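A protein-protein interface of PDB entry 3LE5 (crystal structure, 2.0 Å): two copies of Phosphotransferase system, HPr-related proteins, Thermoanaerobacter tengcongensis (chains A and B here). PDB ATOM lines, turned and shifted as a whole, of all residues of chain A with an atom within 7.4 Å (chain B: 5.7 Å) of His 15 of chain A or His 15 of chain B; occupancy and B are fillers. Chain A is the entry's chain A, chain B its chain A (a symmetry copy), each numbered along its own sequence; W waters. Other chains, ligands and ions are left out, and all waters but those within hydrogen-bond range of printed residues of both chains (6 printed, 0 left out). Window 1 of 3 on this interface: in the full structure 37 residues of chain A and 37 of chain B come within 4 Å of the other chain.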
ATOM      1  N   ILE A   8      38.016  27.784  -1.670  1.00  0.00           N
ATOM      2  CA  ILE A   8      37.405  27.036  -0.570  1.00  0.00           C
ATOM      3  C   ILE A   8      37.371  25.542  -0.897  1.00  0.00           C
ATOM      4  O   ILE A   8      36.649  25.121  -1.794  1.00  0.00           O
ATOM      5  CB  ILE A   8      35.972  27.538  -0.303  1.00  0.00           C
ATOM      6  CG1 ILE A   8      35.968  29.063  -0.147  1.00  0.00           C
ATOM      7  CG2 ILE A   8      35.362  26.830   0.906  1.00  0.00           C
ATOM      8  CD1 ILE A   8      36.808  29.556   1.009  1.00  0.00           C
ATOM      9  N   ASN A  10      37.126  22.711   1.450  1.00  0.00           N
ATOM     10  CA  ASN A  10      36.460  21.758   2.334  1.00  0.00           C
ATOM     11  C   ASN A  10      35.160  21.243   1.727  1.00  0.00           C
ATOM     12  O   ASN A  10      34.590  21.872   0.837  1.00  0.00           O
ATOM     13  CB  ASN A  10      36.195  22.356   3.716  1.00  0.00           C
ATOM     14  CG  ASN A  10      35.054  23.339   3.709  1.00  0.00           C
ATOM     15  OD1 ASN A  10      35.071  24.309   2.957  1.00  0.00           O
ATOM     16  ND2 ASN A  10      34.051  23.098   4.547  1.00  0.00           N
ATOM     17  N   LYS A  11      34.702  20.099   2.227  1.00  0.00           N
ATOM     18  CA  LYS A  11      33.536  19.407   1.682  1.00  0.00           C
ATOM     19  C   LYS A  11      32.364  20.335   1.395  1.00  0.00           C
ATOM     20  O   LYS A  11      32.097  20.670   0.244  1.00  0.00           O
ATOM     21  CB  LYS A  11      33.096  18.281   2.625  1.00  0.00           C
ATOM     22  N   THR A  12      31.686  20.761   2.445  1.00  0.00           N
ATOM     23  CA  THR A  12      30.491  21.573   2.326  1.00  0.00           C
ATOM     24  C   THR A  12      30.767  23.055   2.136  1.00  0.00           C
ATOM     25  O   THR A  12      29.992  23.899   2.549  1.00  0.00           O
ATOM     26  CB  THR A  12      29.587  21.400   3.529  1.00  0.00           C
ATOM     27  OG1 THR A  12      30.353  21.538   4.719  1.00  0.00           O
ATOM     28  N   GLY A  13      31.872  23.370   1.487  1.00  0.00           N
ATOM     29  CA  GLY A  13      32.296  24.741   1.379  1.00  0.00           C
ATOM     30  C   GLY A  13      32.064  25.516   2.647  1.00  0.00           C
ATOM     31  O   GLY A  13      32.678  25.249   3.652  1.00  0.00           O
ATOM     32  N   LEU A  14      31.175  26.488   2.579  1.00  0.00           N
ATOM     33  CA  LEU A  14      30.697  27.174   3.756  1.00  0.00           C
ATOM     34  C   LEU A  14      29.187  27.024   3.897  1.00  0.00           C
ATOM     35  O   LEU A  14      28.511  27.928   4.330  1.00  0.00           O
ATOM     36  CB  LEU A  14      31.092  28.649   3.713  1.00  0.00           C
ATOM     37  CG  LEU A  14      32.573  28.992   3.646  1.00  0.00           C
ATOM     38  CD1 LEU A  14      32.781  30.478   3.573  1.00  0.00           C
ATOM     39  CD2 LEU A  14      33.314  28.429   4.799  1.00  0.00           C
ATOM     40  N   HIS A  15      28.687  25.858   3.518  1.00  0.00           N
ATOM     41  CA  HIS A  15      27.265  25.572   3.511  1.00  0.00           C
ATOM     42  C   HIS A  15      26.722  25.379   4.886  1.00  0.00           C
ATOM     43  O   HIS A  15      27.201  24.568   5.623  1.00  0.00           O
ATOM     44  CB  HIS A  15      26.978  24.329   2.707  1.00  0.00           C
ATOM     45  CG  HIS A  15      26.747  24.594   1.262  1.00  0.00           C
ATOM     46  ND1 HIS A  15      27.694  24.337   0.301  1.00  0.00           N
ATOM     47  CD2 HIS A  15      25.676  25.094   0.609  1.00  0.00           C
ATOM     48  CE1 HIS A  15      27.222  24.674  -0.880  1.00  0.00           C
ATOM     49  NE2 HIS A  15      25.999  25.137  -0.722  1.00  0.00           N
ATOM     50  N   ALA A  16      25.685  26.121   5.196  1.00  0.00           N
ATOM     51  CA  ALA A  16      25.096  26.170   6.518  1.00  0.00           C
ATOM     52  C   ALA A  16      23.622  26.477   6.362  1.00  0.00           C
ATOM     53  O   ALA A  16      22.985  27.003   7.278  1.00  0.00           O
ATOM     54  CB  ALA A  16      25.775  27.232   7.354  1.00  0.00           C
ATOM     55  N   ARG A  17      23.044  26.151   5.222  1.00  0.00           N
ATOM     56  CA  ARG A  17      21.674  26.550   4.972  1.00  0.00           C
ATOM     57  C   ARG A  17      20.719  26.036   6.041  1.00  0.00           C
ATOM     58  O   ARG A  17      19.889  26.762   6.552  1.00  0.00           O
ATOM     59  CB  ARG A  17      21.210  26.102   3.601  1.00  0.00           C
ATOM     60  CG  ARG A  17      20.003  26.828   3.126  1.00  0.00           C
ATOM     61  CD  ARG A  17      19.902  26.772   1.645  1.00  0.00           C
ATOM     62  NE  ARG A  17      18.887  27.666   1.123  1.00  0.00           N
ATOM     63  CZ  ARG A  17      18.563  28.818   1.680  1.00  0.00           C
ATOM     64  NH1 ARG A  17      19.172  29.209   2.785  1.00  0.00           N
ATOM     65  NH2 ARG A  17      17.628  29.573   1.138  1.00  0.00           N
ATOM     66  N   PRO A  18      20.835  24.766   6.363  1.00  0.00           N
ATOM     67  CA  PRO A  18      19.927  24.168   7.323  1.00  0.00           C
ATOM     68  C   PRO A  18      19.790  25.083   8.500  1.00  0.00           C
ATOM     69  O   PRO A  18      18.804  25.752   8.628  1.00  0.00           O
ATOM     70  CB  PRO A  18      20.636  22.885   7.714  1.00  0.00           C
ATOM     71  CG  PRO A  18      22.041  23.127   7.434  1.00  0.00           C
ATOM     72  CD  PRO A  18      22.085  24.013   6.251  1.00  0.00           C
ATOM     73  N   ALA A  19      20.785  25.136   9.354  1.00  0.00           N
ATOM     74  CA  ALA A  19      20.710  26.052  10.450  1.00  0.00           C
ATOM     75  C   ALA A  19      20.247  27.415   9.987  1.00  0.00           C
ATOM     76  O   ALA A  19      19.951  28.281  10.781  1.00  0.00           O
ATOM     77  CB  ALA A  19      21.994  26.134  11.138  1.00  0.00           C
ATOM     78  N   ILE A  50      22.406  26.289  17.526  1.00  0.00           N
ATOM     79  CA  ILE A  50      22.040  25.276  16.554  1.00  0.00           C
ATOM     80  C   ILE A  50      23.303  24.594  16.039  1.00  0.00           C
ATOM     81  O   ILE A  50      23.407  23.365  16.044  1.00  0.00           O
ATOM     82  CB  ILE A  50      21.265  25.883  15.367  1.00  0.00           C
ATOM     83  CG1 ILE A  50      20.072  26.705  15.859  1.00  0.00           C
ATOM     84  CG2 ILE A  50      20.808  24.795  14.414  1.00  0.00           C
ATOM     85  CD1 ILE A  50      19.097  25.923  16.696  1.00  0.00           C
ATOM     86  N   MET A  51      24.267  25.400  15.607  1.00  0.00           N
ATOM     87  CA  MET A  51      25.498  24.870  15.037  1.00  0.00           C
ATOM     88  C   MET A  51      26.267  24.073  16.069  1.00  0.00           C
ATOM     89  O   MET A  51      26.967  23.120  15.730  1.00  0.00           O
ATOM     90  CB  MET A  51      26.373  25.999  14.499  1.00  0.00           C
ATOM     91  CG  MET A  51      25.755  26.750  13.333  1.00  0.00           C
ATOM     92  N   GLY A  54      25.530  20.222  17.185  1.00  0.00           N
ATOM     93  CA  GLY A  54      26.166  19.190  16.387  1.00  0.00           C
ATOM     94  C   GLY A  54      25.152  18.224  15.825  1.00  0.00           C
ATOM     95  O   GLY A  54      25.409  17.024  15.713  1.00  0.00           O
ATOM     96  N   VAL A  55      23.989  18.756  15.475  1.00  0.00           N
ATOM     97  CA  VAL A  55      22.909  17.926  14.981  1.00  0.00           C
ATOM     98  C   VAL A  55      23.160  17.520  13.539  1.00  0.00           C
ATOM     99  O   VAL A  55      23.376  18.357  12.663  1.00  0.00           O
ATOM    100  CB  VAL A  55      21.551  18.615  15.118  1.00  0.00           C
ATOM    101  CG1 VAL A  55      20.458  17.711  14.591  1.00  0.00           C
ATOM    102  CG2 VAL A  55      21.300  18.966  16.574  1.00  0.00           C
ATOM    103  N   SER A  56      23.142  16.211  13.323  1.00  0.00           N
ATOM    104  CA  SER A  56      23.390  15.627  12.019  1.00  0.00           C
ATOM    105  C   SER A  56      22.134  14.924  11.560  1.00  0.00           C
ATOM    106  O   SER A  56      21.212  14.703  12.340  1.00  0.00           O
ATOM    107  CB  SER A  56      24.525  14.603  12.101  1.00  0.00           C
ATOM    108  OG  SER A  56      25.515  14.993  13.040  1.00  0.00           O
ATOM    109  N   GLN A  57      22.106  14.577  10.282  1.00  0.00           N
ATOM    110  CA  GLN A  57      21.059  13.735   9.746  1.00  0.00           C
ATOM    111  C   GLN A  57      20.908  12.526  10.667  1.00  0.00           C
ATOM    112  O   GLN A  57      21.903  11.916  11.050  1.00  0.00           O
ATOM    113  CB  GLN A  57      21.465  13.280   8.352  1.00  0.00           C
ATOM    114  CG  GLN A  57      20.409  12.507   7.604  1.00  0.00           C
ATOM    115  CD  GLN A  57      20.984  11.796   6.398  1.00  0.00           C
ATOM    116  OE1 GLN A  57      22.203  11.758   6.214  1.00  0.00           O
ATOM    117  NE2 GLN A  57      20.114  11.228   5.570  1.00  0.00           N
ATOM    118  N   ASN A  59      19.602  12.511  13.822  1.00  0.00           N
ATOM    119  CA  ASN A  59      19.459  12.897  15.225  1.00  0.00           C
ATOM    120  C   ASN A  59      18.025  13.233  15.616  1.00  0.00           C
ATOM    121  O   ASN A  59      17.308  13.910  14.881  1.00  0.00           O
ATOM    122  CB  ASN A  59      20.374  14.083  15.555  1.00  0.00           C
ATOM    123  CG  ASN A  59      21.627  13.666  16.301  1.00  0.00           C
ATOM    124  OD1 ASN A  59      22.721  14.164  16.028  1.00  0.00           O
ATOM    125  ND2 ASN A  59      21.471  12.755  17.257  1.00  0.00           N
ATOM    126  N   THR B  12      23.097  17.079   5.690  1.00  0.00           N
ATOM    127  CA  THR B  12      24.041  17.602   6.658  1.00  0.00           C
ATOM    128  C   THR B  12      23.424  17.936   8.005  1.00  0.00           C
ATOM    129  O   THR B  12      23.871  18.831   8.700  1.00  0.00           O
ATOM    130  CB  THR B  12      24.747  18.834   6.129  1.00  0.00           C
ATOM    131  OG1 THR B  12      23.784  19.738   5.604  1.00  0.00           O
ATOM    132  N   GLY B  13      22.399  17.196   8.383  1.00  0.00           N
ATOM    133  CA  GLY B  13      21.655  17.522   9.571  1.00  0.00           C
ATOM    134  C   GLY B  13      21.462  19.004   9.741  1.00  0.00           C
ATOM    135  O   GLY B  13      20.781  19.629   8.963  1.00  0.00           O
ATOM    136  N   LEU B  14      22.065  19.554  10.777  1.00  0.00           N
ATOM    137  CA  LEU B  14      22.145  20.985  10.949  1.00  0.00           C
ATOM    138  C   LEU B  14      23.597  21.446  11.005  1.00  0.00           C
ATOM    139  O   LEU B  14      23.931  22.356  11.727  1.00  0.00           O
ATOM    140  CB  LEU B  14      21.391  21.417  12.205  1.00  0.00           C
ATOM    141  CG  LEU B  14      19.904  21.103  12.292  1.00  0.00           C
ATOM    142  CD1 LEU B  14      19.331  21.561  13.603  1.00  0.00           C
ATOM    143  CD2 LEU B  14      19.155  21.710  11.167  1.00  0.00           C
ATOM    144  N   HIS B  15      24.439  20.789  10.223  1.00  0.00           N
ATOM    145  CA  HIS B  15      25.867  21.043  10.210  1.00  0.00           C
ATOM    146  C   HIS B  15      26.205  22.325   9.529  1.00  0.00           C
ATOM    147  O   HIS B  15      25.839  22.537   8.410  1.00  0.00           O
ATOM    148  CB  HIS B  15      26.599  19.925   9.511  1.00  0.00           C
ATOM    149  CG  HIS B  15      26.990  18.811  10.416  1.00  0.00           C
ATOM    150  ND1 HIS B  15      26.316  17.615  10.452  1.00  0.00           N
ATOM    151  CD2 HIS B  15      27.985  18.708  11.321  1.00  0.00           C
ATOM    152  CE1 HIS B  15      26.873  16.825  11.345  1.00  0.00           C
ATOM    153  NE2 HIS B  15      27.888  17.464  11.888  1.00  0.00           N
ATOM    154  N   ALA B  16      26.946  23.158  10.222  1.00  0.00           N
ATOM    155  CA  ALA B  16      27.273  24.499   9.785  1.00  0.00           C
ATOM    156  C   ALA B  16      28.621  24.866  10.370  1.00  0.00           C
ATOM    157  O   ALA B  16      28.937  26.046  10.541  1.00  0.00           O
ATOM    158  CB  ALA B  16      26.211  25.473  10.245  1.00  0.00           C
ATOM    159  N   ARG B  17      29.444  23.883  10.676  1.00  0.00           N
ATOM    160  CA  ARG B  17      30.685  24.175  11.366  1.00  0.00           C
ATOM    161  C   ARG B  17      31.549  25.169  10.603  1.00  0.00           C
ATOM    162  O   ARG B  17      32.064  26.120  11.159  1.00  0.00           O
ATOM    163  CB  ARG B  17      31.471  22.910  11.647  1.00  0.00           C
ATOM    164  CG  ARG B  17      32.509  23.087  12.697  1.00  0.00           C
ATOM    165  CD  ARG B  17      32.865  21.783  13.312  1.00  0.00           C
ATOM    166  NE  ARG B  17      33.684  21.934  14.499  1.00  0.00           N
ATOM    167  CZ  ARG B  17      33.598  22.958  15.327  1.00  0.00           C
ATOM    168  NH1 ARG B  17      32.733  23.927  15.089  1.00  0.00           N
ATOM    169  NH2 ARG B  17      34.380  23.016  16.387  1.00  0.00           N
ATOM    170  N   PRO B  18      31.717  24.931   9.321  1.00  0.00           N
ATOM    171  CA  PRO B  18      32.577  25.784   8.524  1.00  0.00           C
ATOM    172  C   PRO B  18      32.273  27.215   8.840  1.00  0.00           C
ATOM    173  O   PRO B  18      33.015  27.846   9.540  1.00  0.00           O
ATOM    174  CB  PRO B  18      32.173  25.446   7.100  1.00  0.00           C
ATOM    175  CG  PRO B  18      30.820  24.926   7.203  1.00  0.00           C
ATOM    176  CD  PRO B  18      30.744  24.213   8.496  1.00  0.00           C
ATOM    177  N   GLY B  54      26.640  31.505  -0.209  1.00  0.00           N
ATOM    178  CA  GLY B  54      26.438  30.234  -0.877  1.00  0.00           C
ATOM    179  C   GLY B  54      27.748  29.627  -1.317  1.00  0.00           C
ATOM    180  O   GLY B  54      27.835  28.994  -2.371  1.00  0.00           O
ATOM    181  N   VAL B  55      28.773  29.828  -0.500  1.00  0.00           N
ATOM    182  CA  VAL B  55      30.099  29.352  -0.838  1.00  0.00           C
ATOM    183  C   VAL B  55      30.206  27.854  -0.608  1.00  0.00           C
ATOM    184  O   VAL B  55      29.927  27.348   0.479  1.00  0.00           O
ATOM    185  CB  VAL B  55      31.187  30.094  -0.064  1.00  0.00           C
ATOM    186  CG1 VAL B  55      32.550  29.563  -0.450  1.00  0.00           C
ATOM    187  CG2 VAL B  55      31.092  31.583  -0.348  1.00  0.00           C
ATOM    188  N   SER B  56      30.600  27.159  -1.668  1.00  0.00           N
ATOM    189  CA  SER B  56      30.734  25.716  -1.654  1.00  0.00           C
ATOM    190  C   SER B  56      32.189  25.364  -1.866  1.00  0.00           C
ATOM    191  O   SER B  56      32.993  26.210  -2.249  1.00  0.00           O
ATOM    192  CB  SER B  56      29.909  25.094  -2.785  1.00  0.00           C
ATOM    193  OG  SER B  56      28.710  25.817  -3.015  1.00  0.00           O
ATOM    194  N   GLN B  57      32.519  24.108  -1.610  1.00  0.00           N
ATOM    195  CA  GLN B  57      33.823  23.581  -1.946  1.00  0.00           C
ATOM    196  C   GLN B  57      34.130  23.965  -3.391  1.00  0.00           C
ATOM    197  O   GLN B  57      33.279  23.807  -4.264  1.00  0.00           O
ATOM    198  CB  GLN B  57      33.788  22.066  -1.805  1.00  0.00           C
ATOM    199  CG  GLN B  57      35.118  21.381  -1.986  1.00  0.00           C
ATOM    200  CD  GLN B  57      34.958  19.889  -2.182  1.00  0.00           C
ATOM    201  OE1 GLN B  57      33.840  19.393  -2.339  1.00  0.00           O
ATOM    202  NE2 GLN B  57      36.071  19.164  -2.178  1.00  0.00           N
HETATM  203  O   HOH W   1      24.107  15.124   8.697  1.00  0.00           O
HETATM  204  O   HOH W   2      24.023  21.400  14.586  1.00  0.00           O
HETATM  205  O   HOH W   3      29.764  24.968  15.290  1.00  0.00           O
HETATM  206  O   HOH W   4      26.837  21.867   5.943  1.00  0.00           O
HETATM  207  O   HOH W   5      30.737  22.397  -0.766  1.00  0.00           O
HETATM  208  O   HOH W   6      28.198  30.059   2.220  1.00  0.00           O
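His 15 of chain A touches four residues of chain B. His 15 of chain B touches just these residues of chain A: His 15, Pro 18, Val 55 and Ser 56. Of the printed residues of chain A, Leu 14 of chain B touches Pro 18, Ile 50 and Val 55. Of the printed residues of chain B, Val 55 of chain A touches Gly 13 (3.6 Å), Leu 14 (2.6 Å) and His 15 (3.6 Å). Of the printed residues of chain B, Pro 18 of chain A touches Gly 13 (3.5 Å), Leu 14 (3.9 Å) and His 15 (3.97 Å). Of the printed residues of chain B, Lys 11 of chain A touches Gln 57 (3.0 Å). The nearest residue of chain B that does not touch His 15 of chain A is Ala 16 of chain B (4.2 Å). The nearest printed residue of chain B that does not touch Lys 11 of chain A is Ser 56 of chain B (5.1 Å).
Gly 13 of chain A touches Ser 56 of chain B, and with the chains exchanged Ser 56 of chain A touches Gly 13 of chain B. Gly 13 of chain A touches Gln 57 of chain B, and with the chains exchanged Gln 57 of chain A touches Gly 13 of chain B. Leu 14 of chain A touches Pro 18 of chain B, and with the chains exchanged Pro 18 of chain A touches Leu 14 of chain B. His 15 of chain B touches its own counterpart, His 15 of chain A. Of the 28 pairs that touch across the chains among the printed residues, 20 have their exchanged pair printed and touching as well.
The backbone NH of Gly 13 of chain B sits close to the backbone NH of Gln 57 of chain A (3.2 Å). N of Leu 14 of chain B is in hydrogen-bond range of O of Val 55 of chain A (2.6 Å). The backbone carbonyl oxygen (O) of Lys 11 of chain A lies close to the side-chain amide oxygen (OE1) of Gln 57 of chain B, at 3.4 Å. N of Gln 57 of chain B lies close to N of Gly 13 of chain A, 3.2 Å away. The backbone NH (N) of Leu 14 of chain A lies within hydrogen-bond range of the backbone carbonyl oxygen (O) of Val 55 of chain B (2.6 Å).
OG of Ser 56 of chain B sits at hydrogen-bond distance from O of Gly 54 of chain B (3.4 Å). The backbone NH of Ser 56 of chain A is in hydrogen-bond range of the side-chain amide oxygen of Asn 59 of chain A. The backbone carbonyl oxygen (O) of Gly 54 of chain A sits at hydrogen-bond distance from the side-chain hydroxyl (OG) of Ser 56 of chain A, 3.4 Å away. A ring nitrogen (ND1) of His 15 of chain B sits close to the backbone carbonyl oxygen of Thr 12 of chain B, 3.2 Å away. The backbone carbonyl oxygen of Thr 12 of chain A sits close to a ring nitrogen (ND1) of His 15 of chain A, 3.2 Å away. OD1 of Asn 10 of chain A lies close to O of Gly 13 of chain A, at 2.7 Å.
Water W5 lies within hydrogen-bond range of the backbone carbonyl oxygen (O) of Lys 11 of chain A (2.4 Å), the backbone NH (N) of Gln 57 of chain B (2.6 Å) and the backbone NH (N) of Gly 13 of chain A (2.7 Å). Water W2 lies within hydrogen-bond range of O of Ile 50 of chain A (2.5 Å), N of Val 55 of chain A (2.8 Å), O of Leu 14 of chain B (3.0 Å) and N of Gly 54 of chain A (3.2 Å). Water W1 lies within hydrogen-bond range of the backbone NH (N) of Gln 57 of chain A (2.6 Å) and the backbone NH (N) of Gly 13 of chain B (2.7 Å). Water W4 lies within hydrogen-bond range of O of His 15 of chain A (2.7 Å) and O of His 15 of chain B (2.7 Å). Water W6 lies within hydrogen-bond range of N of Val 55 of chain B (2.8 Å), O of Leu 14 of chain A (3.0 Å) and N of Gly 54 of chain B (3.2 Å). Water W3 lies within hydrogen-bond range of the guanidinium group (NH1) of Arg 17 of chain B (3.2 Å) and the backbone carbonyl oxygen (O) of Met 51 of chain A (3.4 Å).
Of the 18 printed residues of chain A, 13 touch a printed residue of chain B. Printed residues of chain A that touch a printed residue of chain B: Ile 8, Asn 10, Lys 11, Gly 13, Leu 14, His 15, Ala 16, Pro 18, Ile 50, Met 51, Val 55, Ser 56 and Gln 57. Hydrophobic or aromatic side chains of chain A within 4 Å of the printed part of chain B: Ile 8, Leu 14, His 15, Ala 16, Pro 18, Ile 50, Met 51 and Val 55. Among the printed residues, no Asp or Glu carboxylate lies within 4 Å of a Lys or Arg side-chain nitrogen of the other chain.
CB of Ile 8 of chain A touches O of Ser 56 of chain B, at 3.8 Å. Gln 57 of chain B touches Asn 10 of chain A. Gly 13 of chain A touches Ser 56 of chain B. His 15 of chain B touches His 15 of chain A (O to O, 3.7 Å). His 15 of chain A touches Val 55 of chain B. Ala 16 of chain B touches Ala 16 of chain A (CB to CB, 3.4 Å). CB of Pro 18 of chain A touches O of Gly 13 of chain B (3.5 Å). His 15 of chain B touches Pro 18 of chain A (O to CG, 3.97 Å). Val 55 of chain A touches Gly 13 of chain B. Ser 56 of chain A touches His 15 of chain B.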
